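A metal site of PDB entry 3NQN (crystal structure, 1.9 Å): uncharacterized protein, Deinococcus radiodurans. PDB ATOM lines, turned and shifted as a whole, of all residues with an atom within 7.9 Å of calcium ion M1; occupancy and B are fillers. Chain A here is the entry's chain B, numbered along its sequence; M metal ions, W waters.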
ATOM      1  N   GLY A   1      18.274  10.876 -23.826  1.00  0.00           N
ATOM      2  CA  GLY A   1      17.380  10.011 -22.999  1.00  0.00           C
ATOM      3  C   GLY A   1      16.618  10.791 -21.937  1.00  0.00           C
ATOM      4  O   GLY A   1      15.760  10.234 -21.232  1.00  0.00           O
ATOM      5  N   MET A   2      16.916  12.084 -21.824  1.00  0.00           N
ATOM      6  CA  MET A   2      16.261  12.937 -20.826  1.00  0.00           C
ATOM      7  C   MET A   2      14.868  13.413 -21.233  1.00  0.00           C
ATOM      8  O   MET A   2      14.155  13.976 -20.402  1.00  0.00           O
ATOM      9  CB  MET A   2      17.132  14.148 -20.513  1.00  0.00           C
ATOM     10  CG  MET A   2      18.390  13.808 -19.772  1.00  0.00           C
ATOM     11  SD  MET A   2      19.160  15.388 -18.965  1.00  0.00           S
ATOM     12  CE  MET A   2      20.642  14.527 -17.991  1.00  0.00           C
ATOM     13  N   ILE A   3      14.477  13.213 -22.493  1.00  0.00           N
ATOM     14  CA  ILE A   3      13.137  13.612 -22.930  1.00  0.00           C
ATOM     15  C   ILE A   3      12.093  12.630 -22.401  1.00  0.00           C
ATOM     16  O   ILE A   3      11.122  13.043 -21.765  1.00  0.00           O
ATOM     17  CB  ILE A   3      13.012  13.738 -24.477  1.00  0.00           C
ATOM     18  CG1 ILE A   3      14.086  14.678 -25.047  1.00  0.00           C
ATOM     19  CG2 ILE A   3      11.597  14.256 -24.836  1.00  0.00           C
ATOM     20  CD1 ILE A   3      13.959  14.944 -26.543  1.00  0.00           C
ATOM     21  N   LEU A   4      12.323  11.321 -22.633  1.00  0.00           N
ATOM     22  CA  LEU A   4      11.348  10.245 -22.245  1.00  0.00           C
ATOM     23  C   LEU A   4      11.609   9.617 -20.847  1.00  0.00           C
ATOM     24  O   LEU A   4      11.040   8.571 -20.505  1.00  0.00           O
ATOM     25  CB  LEU A   4      11.345   9.132 -23.303  1.00  0.00           C
ATOM     26  CG  LEU A   4      10.834   9.573 -24.678  1.00  0.00           C
ATOM     27  CD1 LEU A   4      10.686   8.361 -25.593  1.00  0.00           C
ATOM     28  CD2 LEU A   4       9.480  10.305 -24.562  1.00  0.00           C
ATOM     29  N   SER A   5      12.481  10.233 -20.069  1.00  0.00           N
ATOM     30  CA  SER A   5      12.722   9.788 -18.702  1.00  0.00           C
ATOM     31  C   SER A   5      12.757  10.983 -17.792  1.00  0.00           C
ATOM     32  O   SER A   5      13.091  12.091 -18.212  1.00  0.00           O
ATOM     33  CB  SER A   5      14.034   9.038 -18.594  1.00  0.00           C
ATOM     34  OG  SER A   5      15.120   9.893 -18.850  1.00  0.00           O
ATOM     35  N   ALA A   6      12.402  10.773 -16.535  1.00  0.00           N
ATOM     36  CA  ALA A   6      12.539  11.798 -15.524  1.00  0.00           C
ATOM     37  C   ALA A   6      13.109  11.144 -14.266  1.00  0.00           C
ATOM     38  O   ALA A   6      12.964   9.935 -14.063  1.00  0.00           O
ATOM     39  CB  ALA A   6      11.187  12.445 -15.234  1.00  0.00           C
ATOM     40  N   GLU A   7      13.809  11.932 -13.461  1.00  0.00           N
ATOM     41  CA  GLU A   7      14.407  11.451 -12.211  1.00  0.00           C
ATOM     42  C   GLU A   7      14.173  12.494 -11.139  1.00  0.00           C
ATOM     43  O   GLU A   7      14.252  13.681 -11.401  1.00  0.00           O
ATOM     44  CB  GLU A   7      15.921  11.249 -12.392  1.00  0.00           C
ATOM     45  CG  GLU A   7      16.658  10.617 -11.165  1.00  0.00           C
ATOM     46  CD  GLU A   7      17.062  11.647 -10.031  1.00  0.00           C
ATOM     47  OE1 GLU A   7      17.222  12.855 -10.314  1.00  0.00           O
ATOM     48  OE2 GLU A   7      17.239  11.204  -8.885  1.00  0.00           O
ATOM     49  N   PHE A 111      11.280   7.660 -13.789  1.00  0.00           N
ATOM     50  CA  PHE A 111      10.159   7.437 -14.683  1.00  0.00           C
ATOM     51  C   PHE A 111      10.695   7.250 -16.102  1.00  0.00           C
ATOM     52  O   PHE A 111      11.621   7.957 -16.527  1.00  0.00           O
ATOM     53  CB  PHE A 111       9.216   8.620 -14.677  1.00  0.00           C
ATOM     54  CG  PHE A 111       8.680   8.949 -13.350  1.00  0.00           C
ATOM     55  CD1 PHE A 111       9.397   9.777 -12.480  1.00  0.00           C
ATOM     56  CD2 PHE A 111       7.460   8.450 -12.932  1.00  0.00           C
ATOM     57  CE1 PHE A 111       8.888  10.087 -11.229  1.00  0.00           C
ATOM     58  CE2 PHE A 111       6.951   8.751 -11.695  1.00  0.00           C
ATOM     59  CZ  PHE A 111       7.659   9.557 -10.826  1.00  0.00           C
ATOM     60  N   ALA A 136       4.829  13.794 -23.725  1.00  0.00           N
ATOM     61  CA  ALA A 136       5.165  12.745 -22.764  1.00  0.00           C
ATOM     62  C   ALA A 136       6.228  13.235 -21.764  1.00  0.00           C
ATOM     63  O   ALA A 136       6.097  13.051 -20.543  1.00  0.00           O
ATOM     64  CB  ALA A 136       5.661  11.472 -23.520  1.00  0.00           C
ATOM     65  N   GLY A 137       7.273  13.873 -22.270  1.00  0.00           N
ATOM     66  CA  GLY A 137       8.343  14.398 -21.425  1.00  0.00           C
ATOM     67  C   GLY A 137       7.870  15.430 -20.429  1.00  0.00           C
ATOM     68  O   GLY A 137       8.281  15.404 -19.255  1.00  0.00           O
ATOM     69  N   ARG A 138       6.993  16.345 -20.864  1.00  0.00           N
ATOM     70  CA  ARG A 138       6.438  17.375 -19.973  1.00  0.00           C
ATOM     71  C   ARG A 138       5.655  16.729 -18.839  1.00  0.00           C
ATOM     72  O   ARG A 138       5.734  17.162 -17.698  1.00  0.00           O
ATOM     73  CB  ARG A 138       5.531  18.351 -20.729  1.00  0.00           C
ATOM     74  CG  ARG A 138       6.264  19.297 -21.649  1.00  0.00           C
ATOM     75  CD  ARG A 138       5.385  20.472 -22.105  1.00  0.00           C
ATOM     76  NE  ARG A 138       4.234  20.049 -22.921  1.00  0.00           N
ATOM     77  CZ  ARG A 138       4.275  19.826 -24.248  1.00  0.00           C
ATOM     78  NH1 ARG A 138       5.406  19.974 -24.940  1.00  0.00           N
ATOM     79  NH2 ARG A 138       3.172  19.451 -24.882  1.00  0.00           N
ATOM     80  N   LEU A 140       6.060  13.575 -17.570  1.00  0.00           N
ATOM     81  CA  LEU A 140       6.966  12.887 -16.655  1.00  0.00           C
ATOM     82  C   LEU A 140       7.614  13.899 -15.711  1.00  0.00           C
ATOM     83  O   LEU A 140       7.660  13.678 -14.504  1.00  0.00           O
ATOM     84  CB  LEU A 140       8.046  12.118 -17.407  1.00  0.00           C
ATOM     85  CG  LEU A 140       7.603  10.947 -18.310  1.00  0.00           C
ATOM     86  CD1 LEU A 140       8.855  10.270 -18.911  1.00  0.00           C
ATOM     87  CD2 LEU A 140       6.727   9.918 -17.580  1.00  0.00           C
ATOM     88  N   GLU A 141       8.097  15.003 -16.275  1.00  0.00           N
ATOM     89  CA  GLU A 141       8.723  16.061 -15.455  1.00  0.00           C
ATOM     90  C   GLU A 141       7.756  16.725 -14.471  1.00  0.00           C
ATOM     91  O   GLU A 141       8.164  17.065 -13.355  1.00  0.00           O
ATOM     92  CB  GLU A 141       9.384  17.109 -16.311  1.00  0.00           C
ATOM     93  CG  GLU A 141      10.669  16.640 -16.947  1.00  0.00           C
ATOM     94  CD  GLU A 141      11.742  16.209 -15.906  1.00  0.00           C
ATOM     95  OE1 GLU A 141      11.694  16.661 -14.744  1.00  0.00           O
ATOM     96  OE2 GLU A 141      12.620  15.412 -16.276  1.00  0.00           O
ATOM     97  N   ALA A 144       7.356  14.207 -11.638  1.00  0.00           N
ATOM     98  CA  ALA A 144       8.619  14.158 -10.902  1.00  0.00           C
ATOM     99  C   ALA A 144       8.822  15.361  -9.972  1.00  0.00           C
ATOM    100  O   ALA A 144       9.170  15.185  -8.786  1.00  0.00           O
ATOM    101  CB  ALA A 144       9.809  14.055 -11.891  1.00  0.00           C
ATOM    102  N   LYS A 145       8.617  16.563 -10.510  1.00  0.00           N
ATOM    103  CA  LYS A 145       8.824  17.780  -9.744  1.00  0.00           C
ATOM    104  C   LYS A 145       7.802  17.955  -8.626  1.00  0.00           C
ATOM    105  O   LYS A 145       8.054  18.661  -7.651  1.00  0.00           O
ATOM    106  CB  LYS A 145       8.819  18.989 -10.644  1.00  0.00           C
ATOM    107  CG  LYS A 145      10.117  19.140 -11.503  1.00  0.00           C
ATOM    108  CD  LYS A 145      10.126  20.433 -12.264  1.00  0.00           C
ATOM    109  CE  LYS A 145      11.307  20.535 -13.255  1.00  0.00           C
ATOM    110  NZ  LYS A 145      11.225  19.542 -14.371  1.00  0.00           N
HETATM  111 CA    CA M   1      13.299  14.563 -18.394  1.00  0.00          CA
HETATM  112 CA    CA M   2      14.978  15.897 -12.327  1.00  0.00          CA
HETATM  113  O   HOH W   1      15.283  13.617 -17.790  1.00  0.00           O
HETATM  114  O   HOH W   2      11.133  14.326 -19.473  1.00  0.00           O
HETATM  115  O   HOH W   3      15.181  16.227 -17.932  1.00  0.00           O
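The side-chain carboxylate of Glu 141 is in salt-bridge range of the side-chain amino group of Lys 145. OG of Ser 5 sits at hydrogen-bond distance from O of Gly 1 (2.5 Å).
Within 4 Å of calcium ion M1: Met 2, Ser 5 and Glu 141.
The backbone carbonyl oxygen (O) of Met 2 is bound to calcium ion M1, at 2.3 Å. Calcium ion M1 is bound by water W1. OE2 of Glu 141 binds calcium ion M1. Calcium ion M1 is bound by water W2 (2.4 Å). O of Ser 5 binds calcium ion M1 (2.5 Å). Calcium ion M1 is bound by water W3. Calcium ion M1 has six donor atoms within binding distance.
Water W2 lies within hydrogen-bond range of the backbone carbonyl oxygen of Ile 3 and the backbone carbonyl oxygen of Gly 137.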
